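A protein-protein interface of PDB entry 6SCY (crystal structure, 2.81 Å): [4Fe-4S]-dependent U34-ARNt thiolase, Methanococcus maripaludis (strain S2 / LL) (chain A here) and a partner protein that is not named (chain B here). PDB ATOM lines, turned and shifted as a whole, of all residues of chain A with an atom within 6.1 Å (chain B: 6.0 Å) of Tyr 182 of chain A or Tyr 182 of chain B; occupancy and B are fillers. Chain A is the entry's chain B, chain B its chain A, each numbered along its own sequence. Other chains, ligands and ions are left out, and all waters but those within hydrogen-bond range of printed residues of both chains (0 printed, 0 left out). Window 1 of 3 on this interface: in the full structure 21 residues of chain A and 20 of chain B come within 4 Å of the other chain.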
ATOM      1  N   ALA A 177      -6.384 -24.565  -2.968  1.00  0.00           N
ATOM      2  CA  ALA A 177      -7.238 -24.765  -4.129  1.00  0.00           C
ATOM      3  C   ALA A 177      -8.560 -25.414  -3.760  1.00  0.00           C
ATOM      4  O   ALA A 177      -9.587 -25.019  -4.304  1.00  0.00           O
ATOM      5  CB  ALA A 177      -6.513 -25.584  -5.185  1.00  0.00           C
ATOM      6  N   VAL A 178      -8.540 -26.378  -2.824  1.00  0.00           N
ATOM      7  CA  VAL A 178      -9.724 -27.091  -2.332  1.00  0.00           C
ATOM      8  C   VAL A 178     -10.617 -26.079  -1.625  1.00  0.00           C
ATOM      9  O   VAL A 178     -11.789 -25.958  -1.973  1.00  0.00           O
ATOM     10  CB  VAL A 178      -9.338 -28.300  -1.423  1.00  0.00           C
ATOM     11  CG1 VAL A 178     -10.523 -28.796  -0.609  1.00  0.00           C
ATOM     12  CG2 VAL A 178      -8.745 -29.446  -2.236  1.00  0.00           C
ATOM     13  N   MET A 179     -10.035 -25.313  -0.683  1.00  0.00           N
ATOM     14  CA  MET A 179     -10.716 -24.278   0.086  1.00  0.00           C
ATOM     15  C   MET A 179     -11.277 -23.181  -0.821  1.00  0.00           C
ATOM     16  O   MET A 179     -12.374 -22.702  -0.556  1.00  0.00           O
ATOM     17  CB  MET A 179      -9.777 -23.691   1.151  1.00  0.00           C
ATOM     18  CG  MET A 179     -10.499 -23.004   2.306  1.00  0.00           C
ATOM     19  SD  MET A 179     -11.268 -24.149   3.467  1.00  0.00           S
ATOM     20  CE  MET A 179     -11.111 -23.215   4.963  1.00  0.00           C
ATOM     21  N   MET A 180     -10.546 -22.804  -1.891  1.00  0.00           N
ATOM     22  CA  MET A 180     -10.981 -21.799  -2.871  1.00  0.00           C
ATOM     23  C   MET A 180     -12.231 -22.301  -3.591  1.00  0.00           C
ATOM     24  O   MET A 180     -13.211 -21.570  -3.674  1.00  0.00           O
ATOM     25  CB  MET A 180      -9.868 -21.482  -3.883  1.00  0.00           C
ATOM     26  CG  MET A 180      -8.843 -20.485  -3.374  1.00  0.00           C
ATOM     27  SD  MET A 180      -7.441 -20.213  -4.501  1.00  0.00           S
ATOM     28  CE  MET A 180      -8.152 -19.109  -5.668  1.00  0.00           C
ATOM     29  N   ASN A 181     -12.216 -23.574  -4.042  1.00  0.00           N
ATOM     30  CA  ASN A 181     -13.324 -24.265  -4.713  1.00  0.00           C
ATOM     31  C   ASN A 181     -14.539 -24.382  -3.769  1.00  0.00           C
ATOM     32  O   ASN A 181     -15.677 -24.376  -4.234  1.00  0.00           O
ATOM     33  CB  ASN A 181     -12.854 -25.648  -5.210  1.00  0.00           C
ATOM     34  CG  ASN A 181     -13.937 -26.577  -5.730  1.00  0.00           C
ATOM     35  OD1 ASN A 181     -14.472 -27.415  -4.995  1.00  0.00           O
ATOM     36  ND2 ASN A 181     -14.275 -26.458  -7.008  1.00  0.00           N
ATOM     37  N   TYR A 182     -14.286 -24.461  -2.449  1.00  0.00           N
ATOM     38  CA  TYR A 182     -15.309 -24.535  -1.411  1.00  0.00           C
ATOM     39  C   TYR A 182     -15.951 -23.151  -1.222  1.00  0.00           C
ATOM     40  O   TYR A 182     -17.174 -23.049  -1.296  1.00  0.00           O
ATOM     41  CB  TYR A 182     -14.697 -25.034  -0.086  1.00  0.00           C
ATOM     42  CG  TYR A 182     -14.451 -26.529   0.051  1.00  0.00           C
ATOM     43  CD1 TYR A 182     -14.925 -27.431  -0.900  1.00  0.00           C
ATOM     44  CD2 TYR A 182     -13.787 -27.045   1.160  1.00  0.00           C
ATOM     45  CE1 TYR A 182     -14.723 -28.807  -0.760  1.00  0.00           C
ATOM     46  CE2 TYR A 182     -13.602 -28.418   1.323  1.00  0.00           C
ATOM     47  CZ  TYR A 182     -14.065 -29.295   0.358  1.00  0.00           C
ATOM     48  OH  TYR A 182     -13.865 -30.643   0.521  1.00  0.00           O
ATOM     49  N   ILE A 183     -15.127 -22.088  -1.001  1.00  0.00           N
ATOM     50  CA  ILE A 183     -15.567 -20.692  -0.793  1.00  0.00           C
ATOM     51  C   ILE A 183     -16.298 -20.140  -2.034  1.00  0.00           C
ATOM     52  O   ILE A 183     -17.283 -19.420  -1.885  1.00  0.00           O
ATOM     53  CB  ILE A 183     -14.411 -19.758  -0.303  1.00  0.00           C
ATOM     54  CG1 ILE A 183     -13.798 -20.262   1.025  1.00  0.00           C
ATOM     55  CG2 ILE A 183     -14.886 -18.299  -0.154  1.00  0.00           C
ATOM     56  CD1 ILE A 183     -12.370 -19.870   1.268  1.00  0.00           C
ATOM     57  N   GLU A 184     -15.831 -20.491  -3.244  1.00  0.00           N
ATOM     58  CA  GLU A 184     -16.462 -20.069  -4.497  1.00  0.00           C
ATOM     59  C   GLU A 184     -17.734 -20.875  -4.768  1.00  0.00           C
ATOM     60  O   GLU A 184     -18.625 -20.389  -5.465  1.00  0.00           O
ATOM     61  CB  GLU A 184     -15.489 -20.187  -5.682  1.00  0.00           C
ATOM     62  CG  GLU A 184     -14.415 -19.112  -5.692  1.00  0.00           C
ATOM     63  CD  GLU A 184     -13.246 -19.329  -6.637  1.00  0.00           C
ATOM     64  OE1 GLU A 184     -13.029 -20.479  -7.087  1.00  0.00           O
ATOM     65  OE2 GLU A 184     -12.531 -18.338  -6.913  1.00  0.00           O
ATOM     66  N   GLY A 185     -17.806 -22.081  -4.210  1.00  0.00           N
ATOM     67  CA  GLY A 185     -18.946 -22.975  -4.365  1.00  0.00           C
ATOM     68  C   GLY A 185     -19.026 -23.614  -5.734  1.00  0.00           C
ATOM     69  O   GLY A 185     -20.122 -23.933  -6.206  1.00  0.00           O
ATOM     70  N   ASP A 186     -17.860 -23.811  -6.374  1.00  0.00           N
ATOM     71  CA  ASP A 186     -17.744 -24.415  -7.695  1.00  0.00           C
ATOM     72  C   ASP A 186     -17.897 -25.935  -7.671  1.00  0.00           C
ATOM     73  O   ASP A 186     -17.086 -26.644  -7.066  1.00  0.00           O
ATOM     74  CB  ASP A 186     -16.429 -24.006  -8.373  1.00  0.00           C
ATOM     75  CG  ASP A 186     -16.542 -22.748  -9.206  1.00  0.00           C
ATOM     76  OD1 ASP A 186     -17.000 -22.846 -10.372  1.00  0.00           O
ATOM     77  OD2 ASP A 186     -16.165 -21.663  -8.700  1.00  0.00           O
ATOM     78  N   LEU A 190     -15.382 -28.811  -9.963  1.00  0.00           N
ATOM     79  CA  LEU A 190     -15.228 -30.056  -9.205  1.00  0.00           C
ATOM     80  C   LEU A 190     -15.568 -31.254 -10.108  1.00  0.00           C
ATOM     81  O   LEU A 190     -15.026 -32.341  -9.901  1.00  0.00           O
ATOM     82  CB  LEU A 190     -16.168 -30.025  -7.985  1.00  0.00           C
ATOM     83  CG  LEU A 190     -15.873 -30.988  -6.835  1.00  0.00           C
ATOM     84  CD1 LEU A 190     -16.165 -30.331  -5.508  1.00  0.00           C
ATOM     85  CD2 LEU A 190     -16.701 -32.258  -6.950  1.00  0.00           C
ATOM     86  N   SER A 261      -6.740 -32.809   6.588  1.00  0.00           N
ATOM     87  CA  SER A 261      -8.152 -33.177   6.720  1.00  0.00           C
ATOM     88  C   SER A 261      -9.041 -32.457   5.724  1.00  0.00           C
ATOM     89  O   SER A 261     -10.075 -33.006   5.345  1.00  0.00           O
ATOM     90  CB  SER A 261      -8.656 -32.992   8.145  1.00  0.00           C
ATOM     91  OG  SER A 261      -8.810 -31.629   8.493  1.00  0.00           O
ATOM     92  N   ILE A 262      -8.628 -31.250   5.274  1.00  0.00           N
ATOM     93  CA  ILE A 262      -9.332 -30.477   4.250  1.00  0.00           C
ATOM     94  C   ILE A 262      -9.191 -31.233   2.920  1.00  0.00           C
ATOM     95  O   ILE A 262     -10.195 -31.450   2.239  1.00  0.00           O
ATOM     96  CB  ILE A 262      -8.813 -29.010   4.160  1.00  0.00           C
ATOM     97  CG1 ILE A 262      -9.182 -28.201   5.422  1.00  0.00           C
ATOM     98  CG2 ILE A 262      -9.355 -28.313   2.915  1.00  0.00           C
ATOM     99  CD1 ILE A 262      -8.323 -26.925   5.680  1.00  0.00           C
ATOM    100  N   GLY A 265     -10.682 -34.838   2.881  1.00  0.00           N
ATOM    101  CA  GLY A 265     -12.116 -34.590   2.817  1.00  0.00           C
ATOM    102  C   GLY A 265     -12.600 -34.392   1.399  1.00  0.00           C
ATOM    103  O   GLY A 265     -13.734 -34.749   1.081  1.00  0.00           O
ATOM    104  N   TYR A 266     -11.742 -33.829   0.540  1.00  0.00           N
ATOM    105  CA  TYR A 266     -12.036 -33.584  -0.871  1.00  0.00           C
ATOM    106  C   TYR A 266     -11.809 -34.856  -1.687  1.00  0.00           C
ATOM    107  O   TYR A 266     -12.489 -35.069  -2.692  1.00  0.00           O
ATOM    108  CB  TYR A 266     -11.149 -32.454  -1.404  1.00  0.00           C
ATOM    109  CG  TYR A 266     -11.530 -31.957  -2.781  1.00  0.00           C
ATOM    110  CD1 TYR A 266     -12.475 -30.949  -2.941  1.00  0.00           C
ATOM    111  CD2 TYR A 266     -10.898 -32.444  -3.919  1.00  0.00           C
ATOM    112  CE1 TYR A 266     -12.801 -30.458  -4.205  1.00  0.00           C
ATOM    113  CE2 TYR A 266     -11.221 -31.965  -5.187  1.00  0.00           C
ATOM    114  CZ  TYR A 266     -12.179 -30.975  -5.326  1.00  0.00           C
ATOM    115  OH  TYR A 266     -12.510 -30.495  -6.573  1.00  0.00           O
ATOM    116  N   LEU A 269     -14.765 -37.043  -1.152  1.00  0.00           N
ATOM    117  CA  LEU A 269     -15.867 -36.347  -1.814  1.00  0.00           C
ATOM    118  C   LEU A 269     -15.870 -36.664  -3.306  1.00  0.00           C
ATOM    119  O   LEU A 269     -16.916 -37.000  -3.857  1.00  0.00           O
ATOM    120  CB  LEU A 269     -15.706 -34.830  -1.584  1.00  0.00           C
ATOM    121  CG  LEU A 269     -16.919 -33.938  -1.807  1.00  0.00           C
ATOM    122  CD1 LEU A 269     -17.007 -32.874  -0.735  1.00  0.00           C
ATOM    123  CD2 LEU A 269     -16.866 -33.275  -3.171  1.00  0.00           C
ATOM    124  N   ALA B 177     -21.564 -24.088   9.718  1.00  0.00           N
ATOM    125  CA  ALA B 177     -21.713 -25.540   9.797  1.00  0.00           C
ATOM    126  C   ALA B 177     -21.168 -26.244   8.552  1.00  0.00           C
ATOM    127  O   ALA B 177     -20.535 -27.296   8.676  1.00  0.00           O
ATOM    128  CB  ALA B 177     -23.175 -25.895  10.011  1.00  0.00           C
ATOM    129  N   VAL B 178     -21.387 -25.642   7.362  1.00  0.00           N
ATOM    130  CA  VAL B 178     -20.922 -26.142   6.069  1.00  0.00           C
ATOM    131  C   VAL B 178     -19.396 -26.106   6.085  1.00  0.00           C
ATOM    132  O   VAL B 178     -18.765 -27.131   5.835  1.00  0.00           O
ATOM    133  CB  VAL B 178     -21.537 -25.336   4.891  1.00  0.00           C
ATOM    134  CG1 VAL B 178     -20.775 -25.569   3.597  1.00  0.00           C
ATOM    135  CG2 VAL B 178     -23.010 -25.671   4.698  1.00  0.00           C
ATOM    136  N   MET B 179     -18.817 -24.946   6.452  1.00  0.00           N
ATOM    137  CA  MET B 179     -17.375 -24.726   6.549  1.00  0.00           C
ATOM    138  C   MET B 179     -16.733 -25.663   7.568  1.00  0.00           C
ATOM    139  O   MET B 179     -15.635 -26.149   7.313  1.00  0.00           O
ATOM    140  CB  MET B 179     -17.070 -23.255   6.882  1.00  0.00           C
ATOM    141  CG  MET B 179     -15.672 -22.809   6.492  1.00  0.00           C
ATOM    142  SD  MET B 179     -15.424 -22.586   4.702  1.00  0.00           S
ATOM    143  CE  MET B 179     -14.228 -21.305   4.727  1.00  0.00           C
ATOM    144  N   MET B 180     -17.417 -25.934   8.703  1.00  0.00           N
ATOM    145  CA  MET B 180     -16.937 -26.849   9.747  1.00  0.00           C
ATOM    146  C   MET B 180     -16.826 -28.262   9.168  1.00  0.00           C
ATOM    147  O   MET B 180     -15.788 -28.902   9.322  1.00  0.00           O
ATOM    148  CB  MET B 180     -17.867 -26.832  10.978  1.00  0.00           C
ATOM    149  CG  MET B 180     -17.600 -25.683  11.930  1.00  0.00           C
ATOM    150  SD  MET B 180     -18.779 -25.558  13.312  1.00  0.00           S
ATOM    151  CE  MET B 180     -18.143 -26.790  14.409  1.00  0.00           C
ATOM    152  N   ASN B 181     -17.879 -28.706   8.441  1.00  0.00           N
ATOM    153  CA  ASN B 181     -17.970 -30.007   7.769  1.00  0.00           C
ATOM    154  C   ASN B 181     -16.885 -30.129   6.681  1.00  0.00           C
ATOM    155  O   ASN B 181     -16.408 -31.232   6.411  1.00  0.00           O
ATOM    156  CB  ASN B 181     -19.385 -30.196   7.186  1.00  0.00           C
ATOM    157  CG  ASN B 181     -19.574 -31.391   6.277  1.00  0.00           C
ATOM    158  OD1 ASN B 181     -19.469 -31.290   5.051  1.00  0.00           O
ATOM    159  ND2 ASN B 181     -19.870 -32.548   6.854  1.00  0.00           N
ATOM    160  N   TYR B 182     -16.489 -28.992   6.081  1.00  0.00           N
ATOM    161  CA  TYR B 182     -15.449 -28.909   5.059  1.00  0.00           C
ATOM    162  C   TYR B 182     -14.067 -29.057   5.710  1.00  0.00           C
ATOM    163  O   TYR B 182     -13.296 -29.913   5.276  1.00  0.00           O
ATOM    164  CB  TYR B 182     -15.547 -27.567   4.300  1.00  0.00           C
ATOM    165  CG  TYR B 182     -16.615 -27.451   3.225  1.00  0.00           C
ATOM    166  CD1 TYR B 182     -17.346 -28.563   2.810  1.00  0.00           C
ATOM    167  CD2 TYR B 182     -16.863 -26.241   2.594  1.00  0.00           C
ATOM    168  CE1 TYR B 182     -18.306 -28.465   1.802  1.00  0.00           C
ATOM    169  CE2 TYR B 182     -17.802 -26.134   1.569  1.00  0.00           C
ATOM    170  CZ  TYR B 182     -18.525 -27.246   1.180  1.00  0.00           C
ATOM    171  OH  TYR B 182     -19.446 -27.123   0.171  1.00  0.00           O
ATOM    172  N   ILE B 183     -13.767 -28.240   6.760  1.00  0.00           N
ATOM    173  CA  ILE B 183     -12.489 -28.238   7.501  1.00  0.00           C
ATOM    174  C   ILE B 183     -12.240 -29.597   8.200  1.00  0.00           C
ATOM    175  O   ILE B 183     -11.102 -30.073   8.217  1.00  0.00           O
ATOM    176  CB  ILE B 183     -12.356 -27.016   8.474  1.00  0.00           C
ATOM    177  CG1 ILE B 183     -12.452 -25.677   7.716  1.00  0.00           C
ATOM    178  CG2 ILE B 183     -11.048 -27.071   9.279  1.00  0.00           C
ATOM    179  CD1 ILE B 183     -12.950 -24.514   8.521  1.00  0.00           C
ATOM    180  N   GLU B 184     -13.306 -30.219   8.750  1.00  0.00           N
ATOM    181  CA  GLU B 184     -13.214 -31.526   9.405  1.00  0.00           C
ATOM    182  C   GLU B 184     -13.104 -32.649   8.379  1.00  0.00           C
ATOM    183  O   GLU B 184     -12.566 -33.708   8.687  1.00  0.00           O
ATOM    184  CB  GLU B 184     -14.409 -31.768  10.340  1.00  0.00           C
ATOM    185  CG  GLU B 184     -14.353 -30.957  11.625  1.00  0.00           C
ATOM    186  CD  GLU B 184     -15.627 -30.897  12.449  1.00  0.00           C
ATOM    187  OE1 GLU B 184     -16.719 -31.190  11.910  1.00  0.00           O
ATOM    188  OE2 GLU B 184     -15.527 -30.538  13.645  1.00  0.00           O
ATOM    189  N   GLY B 185     -13.609 -32.407   7.177  1.00  0.00           N
ATOM    190  CA  GLY B 185     -13.580 -33.374   6.086  1.00  0.00           C
ATOM    191  C   GLY B 185     -14.582 -34.495   6.248  1.00  0.00           C
ATOM    192  O   GLY B 185     -14.358 -35.601   5.752  1.00  0.00           O
ATOM    193  N   ASP B 186     -15.698 -34.208   6.939  1.00  0.00           N
ATOM    194  CA  ASP B 186     -16.766 -35.165   7.206  1.00  0.00           C
ATOM    195  C   ASP B 186     -17.669 -35.409   5.998  1.00  0.00           C
ATOM    196  O   ASP B 186     -18.346 -34.492   5.519  1.00  0.00           O
ATOM    197  CB  ASP B 186     -17.588 -34.744   8.435  1.00  0.00           C
ATOM    198  CG  ASP B 186     -17.067 -35.313   9.739  1.00  0.00           C
ATOM    199  OD1 ASP B 186     -17.388 -36.483  10.046  1.00  0.00           O
ATOM    200  OD2 ASP B 186     -16.347 -34.588  10.455  1.00  0.00           O
ATOM    201  N   LEU B 190     -22.117 -35.672   6.128  1.00  0.00           N
ATOM    202  CA  LEU B 190     -22.682 -35.143   4.882  1.00  0.00           C
ATOM    203  C   LEU B 190     -23.689 -36.152   4.305  1.00  0.00           C
ATOM    204  O   LEU B 190     -24.631 -35.745   3.626  1.00  0.00           O
ATOM    205  CB  LEU B 190     -21.543 -34.891   3.875  1.00  0.00           C
ATOM    206  CG  LEU B 190     -21.821 -33.952   2.698  1.00  0.00           C
ATOM    207  CD1 LEU B 190     -20.609 -33.106   2.391  1.00  0.00           C
ATOM    208  CD2 LEU B 190     -22.207 -34.727   1.447  1.00  0.00           C
ATOM    209  N   SER B 261     -22.438 -18.120  -1.304  1.00  0.00           N
ATOM    210  CA  SER B 261     -21.763 -18.998  -2.267  1.00  0.00           C
ATOM    211  C   SER B 261     -21.206 -20.251  -1.618  1.00  0.00           C
ATOM    212  O   SER B 261     -21.109 -21.270  -2.293  1.00  0.00           O
ATOM    213  CB  SER B 261     -20.697 -18.255  -3.064  1.00  0.00           C
ATOM    214  OG  SER B 261     -19.554 -17.963  -2.280  1.00  0.00           O
ATOM    215  N   ILE B 262     -20.869 -20.188  -0.311  1.00  0.00           N
ATOM    216  CA  ILE B 262     -20.400 -21.335   0.471  1.00  0.00           C
ATOM    217  C   ILE B 262     -21.586 -22.304   0.628  1.00  0.00           C
ATOM    218  O   ILE B 262     -21.429 -23.497   0.361  1.00  0.00           O
ATOM    219  CB  ILE B 262     -19.802 -20.907   1.842  1.00  0.00           C
ATOM    220  CG1 ILE B 262     -18.474 -20.147   1.660  1.00  0.00           C
ATOM    221  CG2 ILE B 262     -19.582 -22.119   2.742  1.00  0.00           C
ATOM    222  CD1 ILE B 262     -18.045 -19.258   2.873  1.00  0.00           C
ATOM    223  N   GLY B 265     -23.050 -23.683  -2.716  1.00  0.00           N
ATOM    224  CA  GLY B 265     -22.046 -24.649  -3.133  1.00  0.00           C
ATOM    225  C   GLY B 265     -22.261 -26.002  -2.496  1.00  0.00           C
ATOM    226  O   GLY B 265     -21.948 -27.022  -3.106  1.00  0.00           O
ATOM    227  N   TYR B 266     -22.804 -26.017  -1.273  1.00  0.00           N
ATOM    228  CA  TYR B 266     -23.109 -27.237  -0.528  1.00  0.00           C
ATOM    229  C   TYR B 266     -24.447 -27.820  -0.987  1.00  0.00           C
ATOM    230  O   TYR B 266     -24.623 -29.039  -0.963  1.00  0.00           O
ATOM    231  CB  TYR B 266     -23.150 -26.933   0.974  1.00  0.00           C
ATOM    232  CG  TYR B 266     -23.222 -28.158   1.856  1.00  0.00           C
ATOM    233  CD1 TYR B 266     -22.066 -28.808   2.274  1.00  0.00           C
ATOM    234  CD2 TYR B 266     -24.445 -28.629   2.329  1.00  0.00           C
ATOM    235  CE1 TYR B 266     -22.123 -29.910   3.121  1.00  0.00           C
ATOM    236  CE2 TYR B 266     -24.515 -29.738   3.167  1.00  0.00           C
ATOM    237  CZ  TYR B 266     -23.351 -30.375   3.561  1.00  0.00           C
ATOM    238  OH  TYR B 266     -23.408 -31.461   4.399  1.00  0.00           O
ATOM    239  N   LEU B 269     -23.828 -29.556  -4.194  1.00  0.00           N
ATOM    240  CA  LEU B 269     -22.998 -30.714  -3.851  1.00  0.00           C
ATOM    241  C   LEU B 269     -23.890 -31.859  -3.379  1.00  0.00           C
ATOM    242  O   LEU B 269     -23.740 -32.980  -3.861  1.00  0.00           O
ATOM    243  CB  LEU B 269     -22.012 -30.313  -2.737  1.00  0.00           C
ATOM    244  CG  LEU B 269     -20.803 -31.204  -2.489  1.00  0.00           C
ATOM    245  CD1 LEU B 269     -19.562 -30.364  -2.256  1.00  0.00           C
ATOM    246  CD2 LEU B 269     -21.032 -32.121  -1.294  1.00  0.00           C
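OG of Ser 261 of chain A sits at hydrogen-bond distance from O of Ile 183 of chain B (2.8 Å).
OG of Ser 261 of chain B is in hydrogen-bond range of O of Ile 183 of chain A (2.7 Å).
Tyr 182 of chain A touches just one residue of chain B: Tyr 182.
Tyr 182 of chain B touches one residue of chain A.
Printed residues of chain A within 4 Å of Gly 265 of chain B: Gly 185.
Printed residues of chain A within 4 Å of Leu 269 of chain B: Leu 269 (3.9 Å).
The nearest residue of chain A that does not touch Tyr 182 of chain B is Ile 262 of chain A (4.1 Å).
The nearest printed residue of chain B that does not touch Leu 269 of chain A is Leu 190 of chain B (4.8 Å).
Of the 16 printed residues of chain A, 9 touch a printed residue of chain B.
Printed residues of chain B that touch a printed residue of chain A: Met 179, Tyr 182, Ile 183, Gly 185, Ser 261, Ile 262, Gly 265 and Leu 269.
Among the printed residues, 14 pairs touch across the chains.
Among the printed residues, no Asp or Glu carboxylate lies within 4 Å of a Lys or Arg side-chain nitrogen of the other chain.
Met 179 of chain A touches Met 179 of chain B.
Tyr 182 of chain B touches Tyr 182 of chain A.
Ile 262 of chain B touches Ile 183 of chain A.
CB of Ser 261 of chain B touches O of Glu 184 of chain A, at 3.8 Å.
Gly 185 of chain A touches Ser 261 of chain B.
Gly 185 of chain A touches Gly 265 of chain B (O to CA, 3.7 Å).
Gly 185 of chain B touches Ser 261 of chain A (CA to O, 3.6 Å).
Ile 183 of chain B touches Ile 262 of chain A (O to CG1, 3.9 Å).
Gly 265 of chain A touches Gly 185 of chain B.
Leu 269 of chain B touches Leu 269 of chain A.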
